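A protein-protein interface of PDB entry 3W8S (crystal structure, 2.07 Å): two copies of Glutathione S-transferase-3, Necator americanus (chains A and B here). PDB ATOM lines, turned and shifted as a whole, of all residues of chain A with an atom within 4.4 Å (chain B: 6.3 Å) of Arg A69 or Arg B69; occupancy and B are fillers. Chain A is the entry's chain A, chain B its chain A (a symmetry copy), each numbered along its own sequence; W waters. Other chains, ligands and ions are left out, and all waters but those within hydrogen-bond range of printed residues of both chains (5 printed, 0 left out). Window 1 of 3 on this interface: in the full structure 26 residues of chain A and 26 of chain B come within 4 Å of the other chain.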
ATOM      1  N   PHE A  65       9.845  35.743 -25.798  1.00  0.00           N
ATOM      2  CA  PHE A  65      10.681  34.608 -25.384  1.00  0.00           C
ATOM      3  C   PHE A  65      10.161  33.263 -25.845  1.00  0.00           C
ATOM      4  O   PHE A  65      10.934  32.343 -26.172  1.00  0.00           O
ATOM      5  CB  PHE A  65      10.944  34.599 -23.861  1.00  0.00           C
ATOM      6  CG  PHE A  65      11.776  35.778 -23.433  1.00  0.00           C
ATOM      7  CD1 PHE A  65      11.211  37.044 -23.249  1.00  0.00           C
ATOM      8  CD2 PHE A  65      13.138  35.668 -23.310  1.00  0.00           C
ATOM      9  CE1 PHE A  65      12.007  38.155 -22.867  1.00  0.00           C
ATOM     10  CE2 PHE A  65      13.916  36.744 -22.886  1.00  0.00           C
ATOM     11  CZ  PHE A  65      13.384  37.981 -22.720  1.00  0.00           C
ATOM     12  N   ALA A  66       8.841  33.152 -25.941  1.00  0.00           N
ATOM     13  CA  ALA A  66       8.292  31.905 -26.495  1.00  0.00           C
ATOM     14  C   ALA A  66       8.718  31.752 -27.999  1.00  0.00           C
ATOM     15  O   ALA A  66       9.001  30.622 -28.472  1.00  0.00           O
ATOM     16  CB  ALA A  66       6.778  31.891 -26.306  1.00  0.00           C
ATOM     17  N   ILE A  67       8.678  32.838 -28.754  1.00  0.00           N
ATOM     18  CA  ILE A  67       9.127  32.864 -30.174  1.00  0.00           C
ATOM     19  C   ILE A  67      10.641  32.577 -30.281  1.00  0.00           C
ATOM     20  O   ILE A  67      11.060  31.783 -31.099  1.00  0.00           O
ATOM     21  CB  ILE A  67       8.875  34.249 -30.831  1.00  0.00           C
ATOM     22  CG1 ILE A  67       7.349  34.551 -30.942  1.00  0.00           C
ATOM     23  CG2 ILE A  67       9.471  34.306 -32.242  1.00  0.00           C
ATOM     24  CD1 ILE A  67       7.062  36.092 -30.994  1.00  0.00           C
ATOM     25  N   ALA A  68      11.454  33.252 -29.466  1.00  0.00           N
ATOM     26  CA  ALA A  68      12.906  33.035 -29.554  1.00  0.00           C
ATOM     27  C   ALA A  68      13.195  31.562 -29.287  1.00  0.00           C
ATOM     28  O   ALA A  68      13.994  30.929 -30.000  1.00  0.00           O
ATOM     29  CB  ALA A  68      13.669  33.907 -28.569  1.00  0.00           C
ATOM     30  N   ARG A  69      12.551  31.017 -28.251  1.00  0.00           N
ATOM     31  CA  ARG A  69      12.756  29.604 -27.920  1.00  0.00           C
ATOM     32  C   ARG A  69      12.328  28.674 -29.075  1.00  0.00           C
ATOM     33  O   ARG A  69      13.039  27.738 -29.407  1.00  0.00           O
ATOM     34  CB  ARG A  69      12.060  29.150 -26.565  1.00  0.00           C
ATOM     35  CG  ARG A  69      12.370  27.700 -26.193  1.00  0.00           C
ATOM     36  CD  ARG A  69      11.652  27.249 -24.920  1.00  0.00           C
ATOM     37  NE  ARG A  69      12.022  28.215 -23.899  1.00  0.00           N
ATOM     38  CZ  ARG A  69      11.278  29.206 -23.431  1.00  0.00           C
ATOM     39  NH1 ARG A  69       9.999  29.430 -23.820  1.00  0.00           N
ATOM     40  NH2 ARG A  69      11.865  29.995 -22.591  1.00  0.00           N
ATOM     41  N   PHE A  70      11.153  28.918 -29.609  1.00  0.00           N
ATOM     42  CA  PHE A  70      10.649  28.143 -30.728  1.00  0.00           C
ATOM     43  C   PHE A  70      11.668  28.113 -31.912  1.00  0.00           C
ATOM     44  O   PHE A  70      12.001  27.019 -32.410  1.00  0.00           O
ATOM     45  CB  PHE A  70       9.336  28.737 -31.244  1.00  0.00           C
ATOM     46  CG  PHE A  70       8.787  28.013 -32.476  1.00  0.00           C
ATOM     47  CD1 PHE A  70       8.213  26.748 -32.359  1.00  0.00           C
ATOM     48  CD2 PHE A  70       8.832  28.621 -33.739  1.00  0.00           C
ATOM     49  CE1 PHE A  70       7.728  26.060 -33.494  1.00  0.00           C
ATOM     50  CE2 PHE A  70       8.370  27.938 -34.883  1.00  0.00           C
ATOM     51  CZ  PHE A  70       7.791  26.650 -34.757  1.00  0.00           C
ATOM     52  N   VAL A  71      12.138  29.296 -32.341  1.00  0.00           N
ATOM     53  CA  VAL A  71      13.099  29.430 -33.466  1.00  0.00           C
ATOM     54  C   VAL A  71      14.470  28.820 -33.064  1.00  0.00           C
ATOM     55  O   VAL A  71      15.102  28.065 -33.878  1.00  0.00           O
ATOM     56  CB  VAL A  71      13.203  30.927 -33.878  1.00  0.00           C
ATOM     57  CG1 VAL A  71      14.233  31.155 -34.952  1.00  0.00           C
ATOM     58  CG2 VAL A  71      11.860  31.313 -34.569  1.00  0.00           C
ATOM     59  N   ALA A  72      14.937  29.139 -31.853  1.00  0.00           N
ATOM     60  CA  ALA A  72      16.207  28.575 -31.414  1.00  0.00           C
ATOM     61  C   ALA A  72      16.136  27.045 -31.435  1.00  0.00           C
ATOM     62  O   ALA A  72      17.122  26.420 -31.774  1.00  0.00           O
ATOM     63  CB  ALA A  72      16.581  29.055 -30.031  1.00  0.00           C
ATOM     64  N   LYS A  73      14.999  26.441 -31.063  1.00  0.00           N
ATOM     65  CA  LYS A  73      14.946  24.971 -30.978  1.00  0.00           C
ATOM     66  C   LYS A  73      14.964  24.426 -32.447  1.00  0.00           C
ATOM     67  O   LYS A  73      15.592  23.384 -32.708  1.00  0.00           O
ATOM     68  CB  LYS A  73      13.690  24.397 -30.207  1.00  0.00           C
ATOM     69  CG  LYS A  73      13.740  24.382 -28.615  1.00  0.00           C
ATOM     70  CD  LYS A  73      12.401  23.965 -27.832  1.00  0.00           C
ATOM     71  CE  LYS A  73      12.436  24.109 -26.299  1.00  0.00           C
ATOM     72  NZ  LYS A  73      13.812  24.448 -25.656  1.00  0.00           N
ATOM     73  N   ASP A  89      16.788  28.524 -20.522  1.00  0.00           N
ATOM     74  CA  ASP A  89      15.491  29.153 -20.130  1.00  0.00           C
ATOM     75  C   ASP A  89      15.604  29.909 -18.800  1.00  0.00           C
ATOM     76  O   ASP A  89      15.070  31.000 -18.688  1.00  0.00           O
ATOM     77  CB  ASP A  89      14.438  28.080 -19.946  1.00  0.00           C
ATOM     78  CG  ASP A  89      13.980  27.470 -21.277  1.00  0.00           C
ATOM     79  OD1 ASP A  89      14.343  27.992 -22.347  1.00  0.00           O
ATOM     80  OD2 ASP A  89      13.207  26.487 -21.268  1.00  0.00           O
ATOM     81  N   PHE A 155      20.711  31.065 -27.391  1.00  0.00           N
ATOM     82  CA  PHE A 155      20.087  32.369 -27.376  1.00  0.00           C
ATOM     83  C   PHE A 155      20.226  33.074 -26.003  1.00  0.00           C
ATOM     84  O   PHE A 155      20.068  34.282 -25.931  1.00  0.00           O
ATOM     85  CB  PHE A 155      18.641  32.363 -27.935  1.00  0.00           C
ATOM     86  CG  PHE A 155      17.621  31.686 -27.062  1.00  0.00           C
ATOM     87  CD1 PHE A 155      17.520  30.291 -26.968  1.00  0.00           C
ATOM     88  CD2 PHE A 155      16.708  32.451 -26.347  1.00  0.00           C
ATOM     89  CE1 PHE A 155      16.541  29.662 -26.202  1.00  0.00           C
ATOM     90  CE2 PHE A 155      15.750  31.803 -25.526  1.00  0.00           C
ATOM     91  CZ  PHE A 155      15.674  30.411 -25.437  1.00  0.00           C
ATOM     92  N   ILE B  18       4.613  23.592 -10.411  1.00  0.00           N
ATOM     93  CA  ILE B  18       5.663  22.578 -10.477  1.00  0.00           C
ATOM     94  C   ILE B  18       5.236  21.345  -9.615  1.00  0.00           C
ATOM     95  O   ILE B  18       5.376  20.201 -10.080  1.00  0.00           O
ATOM     96  CB  ILE B  18       7.005  23.126  -9.962  1.00  0.00           C
ATOM     97  CG1 ILE B  18       7.535  24.256 -10.918  1.00  0.00           C
ATOM     98  CG2 ILE B  18       8.056  22.009  -9.839  1.00  0.00           C
ATOM     99  CD1 ILE B  18       8.399  25.290 -10.171  1.00  0.00           C
ATOM    100  N   ILE B  21       2.547  19.358 -11.413  1.00  0.00           N
ATOM    101  CA  ILE B  21       3.105  18.532 -12.502  1.00  0.00           C
ATOM    102  C   ILE B  21       3.685  17.197 -11.980  1.00  0.00           C
ATOM    103  O   ILE B  21       3.377  16.122 -12.537  1.00  0.00           O
ATOM    104  CB  ILE B  21       4.127  19.264 -13.362  1.00  0.00           C
ATOM    105  CG1 ILE B  21       3.447  20.468 -14.080  1.00  0.00           C
ATOM    106  CG2 ILE B  21       4.719  18.307 -14.410  1.00  0.00           C
ATOM    107  CD1 ILE B  21       4.464  21.572 -14.439  1.00  0.00           C
ATOM    108  N   SER B  64      10.916  29.722 -11.830  1.00  0.00           N
ATOM    109  CA  SER B  64       9.768  28.816 -11.723  1.00  0.00           C
ATOM    110  C   SER B  64       9.267  28.378 -13.107  1.00  0.00           C
ATOM    111  O   SER B  64       8.935  27.208 -13.276  1.00  0.00           O
ATOM    112  CB  SER B  64       8.623  29.517 -10.922  1.00  0.00           C
ATOM    113  OG  SER B  64       8.162  30.622 -11.676  1.00  0.00           O
ATOM    114  N   PHE B  65       9.244  29.271 -14.125  1.00  0.00           N
ATOM    115  CA  PHE B  65       8.732  28.793 -15.417  1.00  0.00           C
ATOM    116  C   PHE B  65       9.701  27.906 -16.170  1.00  0.00           C
ATOM    117  O   PHE B  65       9.306  26.951 -16.863  1.00  0.00           O
ATOM    118  CB  PHE B  65       8.239  29.950 -16.315  1.00  0.00           C
ATOM    119  CG  PHE B  65       7.032  30.633 -15.730  1.00  0.00           C
ATOM    120  CD1 PHE B  65       7.151  31.581 -14.709  1.00  0.00           C
ATOM    121  CD2 PHE B  65       5.766  30.269 -16.111  1.00  0.00           C
ATOM    122  CE1 PHE B  65       6.007  32.205 -14.147  1.00  0.00           C
ATOM    123  CE2 PHE B  65       4.641  30.914 -15.599  1.00  0.00           C
ATOM    124  CZ  PHE B  65       4.741  31.823 -14.597  1.00  0.00           C
ATOM    125  N   ALA B  66      10.990  28.170 -15.990  1.00  0.00           N
ATOM    126  CA  ALA B  66      11.973  27.266 -16.607  1.00  0.00           C
ATOM    127  C   ALA B  66      11.864  25.838 -15.963  1.00  0.00           C
ATOM    128  O   ALA B  66      12.016  24.805 -16.667  1.00  0.00           O
ATOM    129  CB  ALA B  66      13.368  27.869 -16.475  1.00  0.00           C
ATOM    130  N   ILE B  67      11.699  25.774 -14.652  1.00  0.00           N
ATOM    131  CA  ILE B  67      11.501  24.496 -13.914  1.00  0.00           C
ATOM    132  C   ILE B  67      10.183  23.810 -14.335  1.00  0.00           C
ATOM    133  O   ILE B  67      10.163  22.624 -14.595  1.00  0.00           O
ATOM    134  CB  ILE B  67      11.429  24.724 -12.378  1.00  0.00           C
ATOM    135  CG1 ILE B  67      12.790  25.243 -11.821  1.00  0.00           C
ATOM    136  CG2 ILE B  67      11.084  23.424 -11.644  1.00  0.00           C
ATOM    137  CD1 ILE B  67      12.604  26.052 -10.490  1.00  0.00           C
ATOM    138  N   ALA B  68       9.083  24.564 -14.373  1.00  0.00           N
ATOM    139  CA  ALA B  68       7.799  23.947 -14.739  1.00  0.00           C
ATOM    140  C   ALA B  68       7.927  23.346 -16.134  1.00  0.00           C
ATOM    141  O   ALA B  68       7.484  22.211 -16.382  1.00  0.00           O
ATOM    142  CB  ALA B  68       6.658  24.952 -14.702  1.00  0.00           C
ATOM    143  N   ARG B  69       8.527  24.113 -17.049  1.00  0.00           N
ATOM    144  CA  ARG B  69       8.705  23.619 -18.418  1.00  0.00           C
ATOM    145  C   ARG B  69       9.576  22.346 -18.461  1.00  0.00           C
ATOM    146  O   ARG B  69       9.244  21.396 -19.155  1.00  0.00           O
ATOM    147  CB  ARG B  69       9.274  24.707 -19.428  1.00  0.00           C
ATOM    148  CG  ARG B  69       9.358  24.196 -20.867  1.00  0.00           C
ATOM    149  CD  ARG B  69       9.960  25.225 -21.825  1.00  0.00           C
ATOM    150  NE  ARG B  69       9.154  26.424 -21.668  1.00  0.00           N
ATOM    151  CZ  ARG B  69       9.478  27.522 -21.000  1.00  0.00           C
ATOM    152  NH1 ARG B  69      10.676  27.701 -20.392  1.00  0.00           N
ATOM    153  NH2 ARG B  69       8.552  28.420 -20.922  1.00  0.00           N
ATOM    154  N   PHE B  70      10.694  22.386 -17.772  1.00  0.00           N
ATOM    155  CA  PHE B  70      11.584  21.242 -17.698  1.00  0.00           C
ATOM    156  C   PHE B  70      10.830  19.956 -17.230  1.00  0.00           C
ATOM    157  O   PHE B  70      10.928  18.908 -17.897  1.00  0.00           O
ATOM    158  CB  PHE B  70      12.723  21.512 -16.711  1.00  0.00           C
ATOM    159  CG  PHE B  70      13.659  20.315 -16.524  1.00  0.00           C
ATOM    160  CD1 PHE B  70      14.559  19.955 -17.525  1.00  0.00           C
ATOM    161  CD2 PHE B  70      13.641  19.575 -15.334  1.00  0.00           C
ATOM    162  CE1 PHE B  70      15.408  18.836 -17.375  1.00  0.00           C
ATOM    163  CE2 PHE B  70      14.467  18.444 -15.177  1.00  0.00           C
ATOM    164  CZ  PHE B  70      15.378  18.081 -16.200  1.00  0.00           C
ATOM    165  N   VAL B  71      10.102  20.053 -16.104  1.00  0.00           N
ATOM    166  CA  VAL B  71       9.343  18.914 -15.526  1.00  0.00           C
ATOM    167  C   VAL B  71       8.174  18.526 -16.471  1.00  0.00           C
ATOM    168  O   VAL B  71       7.940  17.298 -16.735  1.00  0.00           O
ATOM    169  CB  VAL B  71       8.862  19.291 -14.095  1.00  0.00           C
ATOM    170  CG1 VAL B  71       8.002  18.220 -13.479  1.00  0.00           C
ATOM    171  CG2 VAL B  71      10.121  19.325 -13.176  1.00  0.00           C
ATOM    172  N   ALA B  72       7.440  19.530 -16.962  1.00  0.00           N
ATOM    173  CA  ALA B  72       6.345  19.224 -17.874  1.00  0.00           C
ATOM    174  C   ALA B  72       6.875  18.470 -19.096  1.00  0.00           C
ATOM    175  O   ALA B  72       6.193  17.587 -19.578  1.00  0.00           O
ATOM    176  CB  ALA B  72       5.622  20.477 -18.315  1.00  0.00           C
ATOM    177  N   LYS B  73       8.064  18.815 -19.609  1.00  0.00           N
ATOM    178  CA  LYS B  73       8.543  18.170 -20.844  1.00  0.00           C
ATOM    179  C   LYS B  73       8.930  16.698 -20.473  1.00  0.00           C
ATOM    180  O   LYS B  73       8.697  15.779 -21.279  1.00  0.00           O
ATOM    181  CB  LYS B  73       9.769  18.891 -21.536  1.00  0.00           C
ATOM    182  CG  LYS B  73       9.466  20.164 -22.443  1.00  0.00           C
ATOM    183  CD  LYS B  73      10.722  20.998 -22.999  1.00  0.00           C
ATOM    184  CE  LYS B  73      10.394  22.307 -23.742  1.00  0.00           C
ATOM    185  NZ  LYS B  73       8.894  22.584 -24.049  1.00  0.00           N
ATOM    186  N   LYS B  74       9.490  16.472 -19.292  1.00  0.00           N
ATOM    187  CA  LYS B  74       9.869  15.106 -18.858  1.00  0.00           C
ATOM    188  C   LYS B  74       8.620  14.249 -18.773  1.00  0.00           C
ATOM    189  O   LYS B  74       8.655  13.076 -19.137  1.00  0.00           O
ATOM    190  CB  LYS B  74      10.522  15.068 -17.462  1.00  0.00           C
ATOM    191  CG  LYS B  74      11.908  15.685 -17.421  1.00  0.00           C
ATOM    192  CD  LYS B  74      12.987  14.693 -17.898  1.00  0.00           C
ATOM    193  CE  LYS B  74      14.387  15.347 -17.855  1.00  0.00           C
ATOM    194  NZ  LYS B  74      15.400  14.608 -18.697  1.00  0.00           N
ATOM    195  N   ALA B  78       3.861  19.471 -21.606  1.00  0.00           N
ATOM    196  CA  ALA B  78       4.414  20.740 -22.143  1.00  0.00           C
ATOM    197  C   ALA B  78       3.823  21.067 -23.499  1.00  0.00           C
ATOM    198  O   ALA B  78       4.176  22.081 -24.078  1.00  0.00           O
ATOM    199  CB  ALA B  78       5.923  20.604 -22.280  1.00  0.00           C
ATOM    200  N   GLU B  85       3.997  23.328 -28.095  1.00  0.00           N
ATOM    201  CA  GLU B  85       4.861  23.702 -26.977  1.00  0.00           C
ATOM    202  C   GLU B  85       5.068  25.211 -26.918  1.00  0.00           C
ATOM    203  O   GLU B  85       5.077  25.779 -25.838  1.00  0.00           O
ATOM    204  CB  GLU B  85       6.240  22.963 -27.007  1.00  0.00           C
ATOM    205  CG  GLU B  85       6.000  21.482 -26.695  1.00  0.00           C
ATOM    206  CD  GLU B  85       7.268  20.662 -26.402  1.00  0.00           C
ATOM    207  OE1 GLU B  85       8.368  21.052 -26.739  1.00  0.00           O
ATOM    208  OE2 GLU B  85       7.164  19.561 -25.795  1.00  0.00           O
ATOM    209  N   ASP B  89       4.031  27.892 -24.079  1.00  0.00           N
ATOM    210  CA  ASP B  89       4.996  28.915 -23.572  1.00  0.00           C
ATOM    211  C   ASP B  89       4.443  30.339 -23.716  1.00  0.00           C
ATOM    212  O   ASP B  89       4.599  31.133 -22.803  1.00  0.00           O
ATOM    213  CB  ASP B  89       6.277  28.848 -24.376  1.00  0.00           C
ATOM    214  CG  ASP B  89       7.109  27.599 -24.056  1.00  0.00           C
ATOM    215  OD1 ASP B  89       6.787  26.879 -23.095  1.00  0.00           O
ATOM    216  OD2 ASP B  89       8.130  27.351 -24.735  1.00  0.00           O
ATOM    217  N   THR B  92       1.874  30.931 -20.920  1.00  0.00           N
ATOM    218  CA  THR B  92       2.483  31.139 -19.586  1.00  0.00           C
ATOM    219  C   THR B  92       3.255  32.468 -19.511  1.00  0.00           C
ATOM    220  O   THR B  92       3.249  33.106 -18.499  1.00  0.00           O
ATOM    221  CB  THR B  92       3.306  29.928 -19.119  1.00  0.00           C
ATOM    222  OG1 THR B  92       4.399  29.751 -20.007  1.00  0.00           O
ATOM    223  CG2 THR B  92       2.405  28.652 -19.251  1.00  0.00           C
ATOM    224  N   ASP B  93       3.850  32.913 -20.616  1.00  0.00           N
ATOM    225  CA  ASP B  93       4.491  34.226 -20.618  1.00  0.00           C
ATOM    226  C   ASP B  93       3.424  35.347 -20.478  1.00  0.00           C
ATOM    227  O   ASP B  93       3.647  36.358 -19.780  1.00  0.00           O
ATOM    228  CB  ASP B  93       5.309  34.433 -21.902  1.00  0.00           C
ATOM    229  CG  ASP B  93       6.771  33.877 -21.767  1.00  0.00           C
ATOM    230  OD1 ASP B  93       7.167  33.423 -20.648  1.00  0.00           O
ATOM    231  OD2 ASP B  93       7.519  33.931 -22.779  1.00  0.00           O
ATOM    232  N   PHE B 155       0.705  22.381 -18.826  1.00  0.00           N
ATOM    233  CA  PHE B 155       0.896  23.228 -17.670  1.00  0.00           C
ATOM    234  C   PHE B 155       0.329  24.654 -17.884  1.00  0.00           C
ATOM    235  O   PHE B 155       0.102  25.360 -16.915  1.00  0.00           O
ATOM    236  CB  PHE B 155       2.348  23.206 -17.127  1.00  0.00           C
ATOM    237  CG  PHE B 155       3.367  23.887 -17.997  1.00  0.00           C
ATOM    238  CD1 PHE B 155       3.866  23.302 -19.169  1.00  0.00           C
ATOM    239  CD2 PHE B 155       3.877  25.124 -17.623  1.00  0.00           C
ATOM    240  CE1 PHE B 155       4.850  23.907 -19.947  1.00  0.00           C
ATOM    241  CE2 PHE B 155       4.838  25.759 -18.451  1.00  0.00           C
ATOM    242  CZ  PHE B 155       5.314  25.163 -19.622  1.00  0.00           C
HETATM  243  O   HOH W   1      12.884  24.698 -19.255  1.00  0.00           O
HETATM  244  O   HOH W   2       8.236  31.410 -22.828  1.00  0.00           O
HETATM  245  O   HOH W   3       8.642  28.199 -27.260  1.00  0.00           O
HETATM  246  O   HOH W   4       9.953  32.401 -21.452  1.00  0.00           O
HETATM  247  O   HOH W   5       8.049  36.267 -23.587  1.00  0.00           O
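The guanidinium group (NH1) of Arg A69 is in salt-bridge range of the side-chain carboxylate (OD2) of Asp B89.
NH1 of Arg B69 lies within salt-bridge range of OD2 of Asp A89, 2.9 Å away.
The guanidinium group of Arg B69 sits close to the guanidinium group of Arg A69.
The side-chain carboxylate (OD1) of Asp A89 lies within salt-bridge range of the guanidinium group (NE) of Arg A69 (2.8 Å).
OD1 of Asp B89 is in salt-bridge range of NE of Arg B69, 2.8 Å away.
OE1 of Glu B85 is in salt-bridge range of NZ of Lys B73 (3.1 Å).
O of Asp B89 is in hydrogen-bond range of OG1 of Thr B92 (3.1 Å).
Among the printed residues, merely in contact across the chains: Phe A65 with Asp B93 (3.7 Å), Ala A66 with Asp B89 (3.6 Å), Ala A66 with Asp B93 (3.5 Å), Lys A73 with Lys B73 (3.7 Å) and Asp A89 with Ala B66 (3.6 Å).
Arg B69 touches just these residues of chain A: Arg A69 and Asp A89.
Of the printed residues of chain B, Lys A73 touches Lys B73 (3.7 Å).
Of the printed residues of chain A, Ala B66 touches Asp A89.
Printed residues of chain A within 4 Å of Lys B73: Lys A73.
Of the printed residues of chain B, Phe A65 touches Asp B93 (3.7 Å).
Phe B70 touches none of the printed residues of chain A.
The nearest printed residue of chain B that does not touch Arg A69 is Lys B73 (5.2 Å).
The nearest printed residue of chain A that does not touch Arg B69 is Lys A73 (5.2 Å).
The nearest printed residue of chain A that does not touch Lys B73 is Arg A69 (5.2 Å).
Of the 19 printed residues of chain B, 5 touch a printed residue of chain A.
Printed residues of chain B that touch a printed residue of chain A: Ala B66, Arg B69, Lys B73, Asp B89 and Asp B93.
Hydrophobic or aromatic side chains of chain B within 4 Å of the printed part of chain A: Ala B66.
Printed residues of chain A that touch a printed residue of chain B: Phe A65, Ala A66, Arg A69, Lys A73 and Asp A89.
Among the printed residues, 8 pairs touch across the chains.
Among the printed residues, Asp or Glu carboxylates within 4 Å of a Lys or Arg side-chain nitrogen of the other chain: Arg A69 with Asp B89 (2.9 Å) and Asp A89 with Arg B69 (2.9 Å).
Ala A66 touches Asp B89, and with the chains exchanged Asp A89 touches Ala B66.
Arg B69 touches its own counterpart, Arg A69.
Arg A69 touches Asp B89, and with the chains exchanged Asp A89 touches Arg B69.
Lys A73 touches its own counterpart, Lys B73.
Water W5 lies within hydrogen-bond range of OD2 of Asp B93 (2.5 Å) and N of Phe A65 (2.9 Å).
Water W2 bridges OD2 of Asp B93 and NH1 of Arg A69.
Water W1 lies within hydrogen-bond range of the side-chain carboxylate (OD2) of Asp A89 and the backbone carbonyl oxygen (O) of Ala B66.
Water W3 bridges OD2 of Asp B89 (2.7 Å) and O of Ala A66 (2.7 Å).
Water W4 lies within hydrogen-bond range of the side-chain carboxylate (OD1) of Asp B93 and the guanidinium group (NH2) of Arg A69.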
